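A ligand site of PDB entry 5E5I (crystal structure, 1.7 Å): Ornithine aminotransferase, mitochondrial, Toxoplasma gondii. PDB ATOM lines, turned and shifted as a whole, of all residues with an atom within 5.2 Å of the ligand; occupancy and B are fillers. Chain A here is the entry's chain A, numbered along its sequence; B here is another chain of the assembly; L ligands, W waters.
The side-chain carboxylate of Glu 229 lies close to an oxygen (O3) of the ligand, 3.3 Å away. Merely in contact with the ligand: Val 79, Thr 135, Tyr 171, Trp 172, Glu 224, Ile 259 and Gly 314 of chain B. Hydrophobic or aromatic side chains that line the ligand: Tyr 49, Val 79, Ala 137, Tyr 171 and Ile 259. The nearest printed residue that does not touch the ligand is Leu 106 of chain B (4.3 Å).
A carbon (C6) of the ligand is bonded to the side-chain amino group (NZ) of Lys 286 (1.4 Å). An oxygen (O6) of the ligand sits at hydrogen-bond distance from the backbone NH (N) of Thr 316 of chain B. The side-chain hydroxyl of Thr 316 of chain B sits at hydrogen-bond distance from an oxygen (O6) of the ligand (2.6 Å). The side-chain carboxylate (OD2) of Asp 257 sits at hydrogen-bond distance from a nitrogen (N1) of the ligand (2.7 Å). An oxygen (O1) of the ligand lies within hydrogen-bond range of the side-chain hydroxyl (OH) of Tyr 49 (2.7 Å). N of Gly 136 is in hydrogen-bond range of O7 of the ligand (2.7 Å). The backbone NH (N) of Ala 137 lies within hydrogen-bond range of an oxygen (O8) of the ligand (2.9 Å). O4 of the ligand is in hydrogen-bond range of NE2 of Gln 260, at 2.9 Å. An oxygen (O2) of the ligand lies within hydrogen-bond range of the backbone NH (N) of Ser 315 of chain B, 3.1 Å away.
NZ of Lys 286 sits at hydrogen-bond distance from OG1 of Thr 316 of chain B (3.4 Å). OD1 of Asp 257 is in hydrogen-bond range of N of Ile 259 (2.8 Å). The side-chain hydroxyl (OH) of Tyr 49 is in hydrogen-bond range of the backbone NH (N) of Ser 315 of chain B, 3.0 Å away. The side-chain amide nitrogen (NE2) of Gln 260 is in hydrogen-bond range of the side-chain carboxylate (OE2) of Glu 229, 3.3 Å away. The side-chain carboxylate of Glu 224 is in hydrogen-bond range of the backbone NH of Tyr 171 (3.2 Å). The side-chain hydroxyl of Thr 135 lies within hydrogen-bond range of the side-chain carboxylate of Glu 138 of chain B (2.8 Å). The side-chain hydroxyl of Thr 135 is in hydrogen-bond range of the backbone NH of Glu 138 of chain A, at 3.1 Å.
Water W3 lies within hydrogen-bond range of O7 of the ligand (2.8 Å), N of Phe 317 of chain B (2.9 Å), OG of Ser 315 of chain B (3.4 Å) and N of Thr 316 of chain B (3.5 Å). Water W9 lies within hydrogen-bond range of OE2 of Glu 138 of chain B (2.7 Å), OG of Ser 315 of chain B (2.8 Å) and O8 of the ligand (2.9 Å). Water W7 lies within hydrogen-bond range of N of Arg 107 of chain B (2.9 Å), O1 of the ligand (2.9 Å), O of Ser 315 of chain B (2.9 Å), OH of Tyr 49 (3.3 Å) and O of Thr 316 of chain B (3.3 Å). Water W11 bridges OH of Tyr 171 (2.5 Å) and O2 of the ligand (2.9 Å). Water W6 lies within hydrogen-bond range of N of Lys 286 (2.8 Å), O7 of the ligand (3.0 Å) and N of Gly 136 (3.5 Å). Water W1 lies within hydrogen-bond range of O2 of the ligand (3.0 Å) and OH of Tyr 171 (3.2 Å).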
ATOM      1  N   TYR A  49     -14.904 -19.251 -11.645  1.00  0.00           N
ATOM      2  CA  TYR A  49     -14.785 -18.110 -10.738  1.00  0.00           C
ATOM      3  C   TYR A  49     -13.321 -17.966 -10.294  1.00  0.00           C
ATOM      4  O   TYR A  49     -12.620 -18.956 -10.086  1.00  0.00           O
ATOM      5  CB  TYR A  49     -15.647 -18.278  -9.484  1.00  0.00           C
ATOM      6  CG  TYR A  49     -17.104 -17.898  -9.713  1.00  0.00           C
ATOM      7  CD1 TYR A  49     -17.988 -18.764 -10.381  1.00  0.00           C
ATOM      8  CD2 TYR A  49     -17.588 -16.640  -9.303  1.00  0.00           C
ATOM      9  CE1 TYR A  49     -19.324 -18.386 -10.614  1.00  0.00           C
ATOM     10  CE2 TYR A  49     -18.905 -16.272  -9.544  1.00  0.00           C
ATOM     11  CZ  TYR A  49     -19.752 -17.148 -10.195  1.00  0.00           C
ATOM     12  OH  TYR A  49     -21.055 -16.778 -10.466  1.00  0.00           O
ATOM     13  N   GLY A  78     -24.523 -11.159  -1.579  1.00  0.00           N
ATOM     14  CA  GLY A  78     -25.069 -11.852  -2.715  1.00  0.00           C
ATOM     15  C   GLY A  78     -25.405 -10.959  -3.881  1.00  0.00           C
ATOM     16  O   GLY A  78     -26.206 -11.340  -4.767  1.00  0.00           O
ATOM     17  N   VAL A  79     -24.699  -9.846  -3.923  1.00  0.00           N
ATOM     18  CA  VAL A  79     -24.936  -8.710  -4.844  1.00  0.00           C
ATOM     19  C   VAL A  79     -26.420  -8.274  -4.665  1.00  0.00           C
ATOM     20  O   VAL A  79     -27.198  -8.197  -5.608  1.00  0.00           O
ATOM     21  CB  VAL A  79     -24.569  -9.006  -6.304  1.00  0.00           C
ATOM     22  CG1 VAL A  79     -24.506  -7.696  -7.086  1.00  0.00           C
ATOM     23  CG2 VAL A  79     -23.201  -9.674  -6.449  1.00  0.00           C
ATOM     24  N   THR A 135     -34.307 -18.105 -11.669  1.00  0.00           N
ATOM     25  CA  THR A 135     -33.157 -17.244 -11.615  1.00  0.00           C
ATOM     26  C   THR A 135     -33.398 -15.909 -12.319  1.00  0.00           C
ATOM     27  O   THR A 135     -34.352 -15.762 -13.074  1.00  0.00           O
ATOM     28  CB  THR A 135     -31.974 -17.938 -12.298  1.00  0.00           C
ATOM     29  OG1 THR A 135     -32.196 -18.064 -13.729  1.00  0.00           O
ATOM     30  CG2 THR A 135     -31.700 -19.300 -11.696  1.00  0.00           C
ATOM     31  N   GLY A 136     -32.457 -14.975 -12.123  1.00  0.00           N
ATOM     32  CA  GLY A 136     -32.534 -13.706 -12.751  1.00  0.00           C
ATOM     33  C   GLY A 136     -32.477 -13.851 -14.272  1.00  0.00           C
ATOM     34  O   GLY A 136     -33.286 -13.217 -15.002  1.00  0.00           O
ATOM     35  N   ALA A 137     -31.589 -14.713 -14.711  1.00  0.00           N
ATOM     36  CA  ALA A 137     -31.438 -14.953 -16.193  1.00  0.00           C
ATOM     37  C   ALA A 137     -32.731 -15.452 -16.767  1.00  0.00           C
ATOM     38  O   ALA A 137     -33.116 -15.094 -17.846  1.00  0.00           O
ATOM     39  CB  ALA A 137     -30.354 -15.984 -16.426  1.00  0.00           C
ATOM     40  N   GLU A 138     -33.419 -16.364 -16.062  1.00  0.00           N
ATOM     41  CA  GLU A 138     -34.673 -16.889 -16.561  1.00  0.00           C
ATOM     42  C   GLU A 138     -35.730 -15.795 -16.606  1.00  0.00           C
ATOM     43  O   GLU A 138     -36.599 -15.861 -17.416  1.00  0.00           O
ATOM     44  CB  GLU A 138     -35.206 -18.067 -15.698  1.00  0.00           C
ATOM     45  CG  GLU A 138     -34.526 -19.369 -15.971  1.00  0.00           C
ATOM     46  CD  GLU A 138     -35.107 -20.540 -15.188  1.00  0.00           C
ATOM     47  OE1 GLU A 138     -35.786 -20.297 -14.134  1.00  0.00           O
ATOM     48  OE2 GLU A 138     -34.861 -21.690 -15.667  1.00  0.00           O
ATOM     49  N   TYR A 171     -25.993  -6.242 -17.688  1.00  0.00           N
ATOM     50  CA  TYR A 171     -25.801  -7.595 -17.228  1.00  0.00           C
ATOM     51  C   TYR A 171     -27.188  -8.108 -16.849  1.00  0.00           C
ATOM     52  O   TYR A 171     -27.838  -7.455 -16.109  1.00  0.00           O
ATOM     53  CB  TYR A 171     -24.904  -7.702 -16.027  1.00  0.00           C
ATOM     54  CG  TYR A 171     -24.637  -9.128 -15.646  1.00  0.00           C
ATOM     55  CD1 TYR A 171     -25.533  -9.855 -14.876  1.00  0.00           C
ATOM     56  CD2 TYR A 171     -23.476  -9.750 -16.042  1.00  0.00           C
ATOM     57  CE1 TYR A 171     -25.275 -11.154 -14.528  1.00  0.00           C
ATOM     58  CE2 TYR A 171     -23.201 -11.071 -15.724  1.00  0.00           C
ATOM     59  CZ  TYR A 171     -24.094 -11.757 -14.939  1.00  0.00           C
ATOM     60  OH  TYR A 171     -23.815 -13.038 -14.606  1.00  0.00           O
ATOM     61  N   TRP A 172     -27.621  -9.220 -17.414  1.00  0.00           N
ATOM     62  CA  TRP A 172     -28.890  -9.817 -17.040  1.00  0.00           C
ATOM     63  C   TRP A 172     -28.820 -11.331 -16.921  1.00  0.00           C
ATOM     64  O   TRP A 172     -29.779 -11.959 -16.505  1.00  0.00           O
ATOM     65  CB  TRP A 172     -30.023  -9.386 -17.944  1.00  0.00           C
ATOM     66  CG  TRP A 172     -30.006  -9.759 -19.366  1.00  0.00           C
ATOM     67  CD1 TRP A 172     -29.499  -9.010 -20.370  1.00  0.00           C
ATOM     68  CD2 TRP A 172     -30.536 -10.936 -19.966  1.00  0.00           C
ATOM     69  NE1 TRP A 172     -29.690  -9.657 -21.587  1.00  0.00           N
ATOM     70  CE2 TRP A 172     -30.304 -10.840 -21.370  1.00  0.00           C
ATOM     71  CE3 TRP A 172     -31.120 -12.108 -19.468  1.00  0.00           C
ATOM     72  CZ2 TRP A 172     -30.733 -11.799 -22.252  1.00  0.00           C
ATOM     73  CZ3 TRP A 172     -31.512 -13.065 -20.324  1.00  0.00           C
ATOM     74  CH2 TRP A 172     -31.313 -12.918 -21.732  1.00  0.00           C
ATOM     75  N   GLY A 173     -27.675 -11.894 -17.249  1.00  0.00           N
ATOM     76  CA  GLY A 173     -27.534 -13.331 -17.170  1.00  0.00           C
ATOM     77  C   GLY A 173     -26.419 -13.930 -17.930  1.00  0.00           C
ATOM     78  O   GLY A 173     -25.609 -13.228 -18.516  1.00  0.00           O
ATOM     79  N   GLU A 224     -31.565  -1.307 -16.676  1.00  0.00           N
ATOM     80  CA  GLU A 224     -31.362  -1.331 -15.217  1.00  0.00           C
ATOM     81  C   GLU A 224     -31.510   0.140 -14.741  1.00  0.00           C
ATOM     82  O   GLU A 224     -30.949   1.025 -15.329  1.00  0.00           O
ATOM     83  CB  GLU A 224     -29.942  -1.831 -14.874  1.00  0.00           C
ATOM     84  CG  GLU A 224     -29.676  -3.255 -15.339  1.00  0.00           C
ATOM     85  CD  GLU A 224     -28.219  -3.664 -15.210  1.00  0.00           C
ATOM     86  OE1 GLU A 224     -27.778  -3.916 -14.041  1.00  0.00           O
ATOM     87  OE2 GLU A 224     -27.588  -3.812 -16.301  1.00  0.00           O
ATOM     88  N   GLU A 229     -23.651  -4.839 -12.299  1.00  0.00           N
ATOM     89  CA  GLU A 229     -22.344  -5.409 -12.635  1.00  0.00           C
ATOM     90  C   GLU A 229     -21.531  -4.417 -13.478  1.00  0.00           C
ATOM     91  O   GLU A 229     -20.292  -4.437 -13.442  1.00  0.00           O
ATOM     92  CB  GLU A 229     -22.482  -6.741 -13.367  1.00  0.00           C
ATOM     93  CG  GLU A 229     -23.270  -7.788 -12.556  1.00  0.00           C
ATOM     94  CD  GLU A 229     -22.667  -8.093 -11.196  1.00  0.00           C
ATOM     95  OE1 GLU A 229     -21.562  -8.698 -11.160  1.00  0.00           O
ATOM     96  OE2 GLU A 229     -23.314  -7.768 -10.165  1.00  0.00           O
ATOM     97  N   ASP A 257     -35.222  -4.017 -15.196  1.00  0.00           N
ATOM     98  CA  ASP A 257     -34.584  -5.072 -14.451  1.00  0.00           C
ATOM     99  C   ASP A 257     -34.259  -4.537 -13.085  1.00  0.00           C
ATOM    100  O   ASP A 257     -33.345  -3.740 -12.926  1.00  0.00           O
ATOM    101  CB  ASP A 257     -33.322  -5.590 -15.173  1.00  0.00           C
ATOM    102  CG  ASP A 257     -32.695  -6.756 -14.480  1.00  0.00           C
ATOM    103  OD1 ASP A 257     -33.007  -6.993 -13.256  1.00  0.00           O
ATOM    104  OD2 ASP A 257     -31.796  -7.436 -15.065  1.00  0.00           O
ATOM    105  N   ILE A 259     -33.720  -6.688 -10.585  1.00  0.00           N
ATOM    106  CA  ILE A 259     -33.194  -7.887  -9.869  1.00  0.00           C
ATOM    107  C   ILE A 259     -32.163  -7.516  -8.777  1.00  0.00           C
ATOM    108  O   ILE A 259     -32.132  -8.111  -7.655  1.00  0.00           O
ATOM    109  CB  ILE A 259     -32.663  -8.916 -10.883  1.00  0.00           C
ATOM    110  CG1 ILE A 259     -33.869  -9.467 -11.650  1.00  0.00           C
ATOM    111  CG2 ILE A 259     -31.908 -10.025 -10.193  1.00  0.00           C
ATOM    112  CD1 ILE A 259     -33.540 -10.194 -12.923  1.00  0.00           C
ATOM    113  N   GLN A 260     -31.296  -6.554  -9.107  1.00  0.00           N
ATOM    114  CA  GLN A 260     -30.283  -6.066  -8.167  1.00  0.00           C
ATOM    115  C   GLN A 260     -30.729  -4.763  -7.489  1.00  0.00           C
ATOM    116  O   GLN A 260     -30.411  -4.554  -6.321  1.00  0.00           O
ATOM    117  CB  GLN A 260     -28.936  -5.872  -8.854  1.00  0.00           C
ATOM    118  CG  GLN A 260     -27.849  -5.361  -7.892  1.00  0.00           C
ATOM    119  CD  GLN A 260     -26.458  -5.327  -8.451  1.00  0.00           C
ATOM    120  OE1 GLN A 260     -25.642  -4.539  -7.970  1.00  0.00           O
ATOM    121  NE2 GLN A 260     -26.152  -6.166  -9.448  1.00  0.00           N
ATOM    122  N   LYS A 286     -33.146 -12.223  -6.849  1.00  0.00           N
ATOM    123  CA  LYS A 286     -32.234 -12.048  -5.715  1.00  0.00           C
ATOM    124  C   LYS A 286     -32.871 -11.951  -4.284  1.00  0.00           C
ATOM    125  O   LYS A 286     -33.255 -12.983  -3.758  1.00  0.00           O
ATOM    126  CB  LYS A 286     -31.296 -10.895  -6.054  1.00  0.00           C
ATOM    127  CG  LYS A 286     -30.284 -11.260  -7.134  1.00  0.00           C
ATOM    128  CD  LYS A 286     -29.279 -10.143  -7.466  1.00  0.00           C
ATOM    129  CE  LYS A 286     -28.068 -10.528  -8.366  1.00  0.00           C
ATOM    130  NZ  LYS A 286     -28.141 -10.754  -9.926  1.00  0.00           N
ATOM    131  N   LEU B 106     -22.343 -16.641  -2.676  1.00  0.00           N
ATOM    132  CA  LEU B 106     -21.926 -16.377  -4.058  1.00  0.00           C
ATOM    133  C   LEU B 106     -20.597 -17.167  -4.238  1.00  0.00           C
ATOM    134  O   LEU B 106     -19.918 -17.504  -3.241  1.00  0.00           O
ATOM    135  CB  LEU B 106     -21.613 -14.939  -4.384  1.00  0.00           C
ATOM    136  CG  LEU B 106     -22.722 -13.909  -4.369  1.00  0.00           C
ATOM    137  CD1 LEU B 106     -22.094 -12.593  -4.748  1.00  0.00           C
ATOM    138  CD2 LEU B 106     -23.857 -14.247  -5.359  1.00  0.00           C
ATOM    139  N   ARG B 107     -20.243 -17.482  -5.476  1.00  0.00           N
ATOM    140  CA  ARG B 107     -18.983 -18.153  -5.733  1.00  0.00           C
ATOM    141  C   ARG B 107     -17.848 -17.133  -5.681  1.00  0.00           C
ATOM    142  O   ARG B 107     -16.675 -17.482  -5.802  1.00  0.00           O
ATOM    143  CB  ARG B 107     -19.037 -19.008  -6.995  1.00  0.00           C
ATOM    144  CG  ARG B 107     -19.828 -20.282  -6.706  1.00  0.00           C
ATOM    145  CD  ARG B 107     -19.769 -21.261  -7.868  1.00  0.00           C
ATOM    146  NE  ARG B 107     -18.390 -21.562  -8.177  1.00  0.00           N
ATOM    147  CZ  ARG B 107     -17.982 -22.035  -9.360  1.00  0.00           C
ATOM    148  NH1 ARG B 107     -18.858 -22.397 -10.282  1.00  0.00           N
ATOM    149  NH2 ARG B 107     -16.698 -22.175  -9.587  1.00  0.00           N
ATOM    150  N   GLU B 138     -30.760 -24.038 -17.452  1.00  0.00           N
ATOM    151  CA  GLU B 138     -29.428 -23.473 -17.228  1.00  0.00           C
ATOM    152  C   GLU B 138     -28.277 -24.527 -17.447  1.00  0.00           C
ATOM    153  O   GLU B 138     -27.171 -24.151 -17.917  1.00  0.00           O
ATOM    154  CB  GLU B 138     -29.308 -22.849 -15.842  1.00  0.00           C
ATOM    155  CG  GLU B 138     -30.013 -21.529 -15.695  1.00  0.00           C
ATOM    156  CD  GLU B 138     -29.816 -20.878 -14.336  1.00  0.00           C
ATOM    157  OE1 GLU B 138     -29.464 -21.608 -13.353  1.00  0.00           O
ATOM    158  OE2 GLU B 138     -29.923 -19.604 -14.322  1.00  0.00           O
ATOM    159  N   GLY B 314     -21.194 -17.777 -14.912  1.00  0.00           N
ATOM    160  CA  GLY B 314     -21.560 -17.512 -13.524  1.00  0.00           C
ATOM    161  C   GLY B 314     -23.050 -17.730 -13.293  1.00  0.00           C
ATOM    162  O   GLY B 314     -23.773 -18.161 -14.201  1.00  0.00           O
ATOM    163  N   SER B 315     -23.476 -17.473 -12.070  1.00  0.00           N
ATOM    164  CA  SER B 315     -24.874 -17.596 -11.625  1.00  0.00           C
ATOM    165  C   SER B 315     -24.906 -17.213 -10.166  1.00  0.00           C
ATOM    166  O   SER B 315     -24.110 -17.731  -9.397  1.00  0.00           O
ATOM    167  CB  SER B 315     -25.313 -19.075 -11.700  1.00  0.00           C
ATOM    168  OG  SER B 315     -26.549 -19.303 -11.045  1.00  0.00           O
ATOM    169  N   THR B 316     -25.860 -16.364  -9.763  1.00  0.00           N
ATOM    170  CA  THR B 316     -25.969 -15.932  -8.403  1.00  0.00           C
ATOM    171  C   THR B 316     -26.134 -17.108  -7.466  1.00  0.00           C
ATOM    172  O   THR B 316     -25.323 -17.313  -6.543  1.00  0.00           O
ATOM    173  CB  THR B 316     -27.142 -14.933  -8.219  1.00  0.00           C
ATOM    174  OG1 THR B 316     -26.900 -13.805  -9.071  1.00  0.00           O
ATOM    175  CG2 THR B 316     -27.301 -14.487  -6.761  1.00  0.00           C
ATOM    176  N   PHE B 317     -27.145 -17.923  -7.738  1.00  0.00           N
ATOM    177  CA  PHE B 317     -27.511 -19.041  -6.840  1.00  0.00           C
ATOM    178  C   PHE B 317     -26.824 -20.363  -7.121  1.00  0.00           C
ATOM    179  O   PHE B 317     -26.967 -21.308  -6.345  1.00  0.00           O
ATOM    180  CB  PHE B 317     -29.043 -19.214  -6.767  1.00  0.00           C
ATOM    181  CG  PHE B 317     -29.744 -18.143  -5.915  1.00  0.00           C
ATOM    182  CD1 PHE B 317     -29.932 -18.340  -4.573  1.00  0.00           C
ATOM    183  CD2 PHE B 317     -30.189 -16.969  -6.461  1.00  0.00           C
ATOM    184  CE1 PHE B 317     -30.527 -17.356  -3.803  1.00  0.00           C
ATOM    185  CE2 PHE B 317     -30.803 -15.974  -5.697  1.00  0.00           C
ATOM    186  CZ  PHE B 317     -30.977 -16.187  -4.343  1.00  0.00           C
HETATM  187  O1  LIG L   1     -22.025 -14.540  -9.246  1.00  0.00           O
HETATM  188  C1  LIG L   1     -22.763 -13.990 -10.105  1.00  0.00           C
HETATM  189  O2  LIG L   1     -23.005 -14.521 -11.202  1.00  0.00           O
HETATM  190  C2  LIG L   1     -23.336 -12.631  -9.756  1.00  0.00           C
HETATM  191  C3  LIG L   1     -24.288 -11.997 -10.778  1.00  0.00           C
HETATM  192  C4  LIG L   1     -25.049 -10.977 -10.333  1.00  0.00           C
HETATM  193  O3  LIG L   1     -24.758 -10.510  -8.952  1.00  0.00           O
HETATM  194  C5  LIG L   1     -26.061 -10.386 -11.032  1.00  0.00           C
HETATM  195  C6  LIG L   1     -27.274 -10.837 -10.987  1.00  0.00           C
HETATM  196  C7  LIG L   1     -28.278 -10.189 -11.940  1.00  0.00           C
HETATM  197  C8  LIG L   1     -28.468  -8.816 -11.903  1.00  0.00           C
HETATM  198  O4  LIG L   1     -27.774  -8.026 -11.027  1.00  0.00           O
HETATM  199  C9  LIG L   1     -29.396  -8.205 -12.750  1.00  0.00           C
HETATM  200  C10 LIG L   1     -29.590  -6.701 -12.632  1.00  0.00           C
HETATM  201  N1  LIG L   1     -30.142  -8.935 -13.620  1.00  0.00           N
HETATM  202  C11 LIG L   1     -29.946 -10.255 -13.728  1.00  0.00           C
HETATM  203  C12 LIG L   1     -29.023 -10.895 -12.902  1.00  0.00           C
HETATM  204  C13 LIG L   1     -28.910 -12.397 -13.084  1.00  0.00           C
HETATM  205  O5  LIG L   1     -29.533 -13.104 -12.033  1.00  0.00           O
HETATM  206  P1  LIG L   1     -29.059 -14.619 -11.766  1.00  0.00           P
HETATM  207  O6  LIG L   1     -27.614 -14.602 -11.415  1.00  0.00           O
HETATM  208  O7  LIG L   1     -30.086 -15.073 -10.758  1.00  0.00           O
HETATM  209  O8  LIG L   1     -29.345 -15.367 -13.054  1.00  0.00           O
HETATM  210  O   HOH W   1     -21.020 -13.339 -13.128  1.00  0.00           O
HETATM  211  O   HOH W   2     -31.399  -4.263 -11.026  1.00  0.00           O
HETATM  212  O   HOH W   3     -29.149 -17.522  -9.834  1.00  0.00           O
HETATM  213  O   HOH W   4     -28.912  -3.456 -11.755  1.00  0.00           O
HETATM  214  O   HOH W   5     -20.265 -13.008  -7.814  1.00  0.00           O
HETATM  215  O   HOH W   6     -31.972 -13.736  -8.904  1.00  0.00           O
HETATM  216  O   HOH W   7     -22.210 -16.763  -7.427  1.00  0.00           O
HETATM  217  O   HOH W   8     -27.108 -15.871 -14.895  1.00  0.00           O
HETATM  218  O   HOH W   9     -28.504 -18.073 -12.610  1.00  0.00           O
HETATM  219  O   HOH W  10     -26.202  -6.101 -13.121  1.00  0.00           O
HETATM  220  O   HOH W  11     -25.217 -14.478 -13.051  1.00  0.00           O
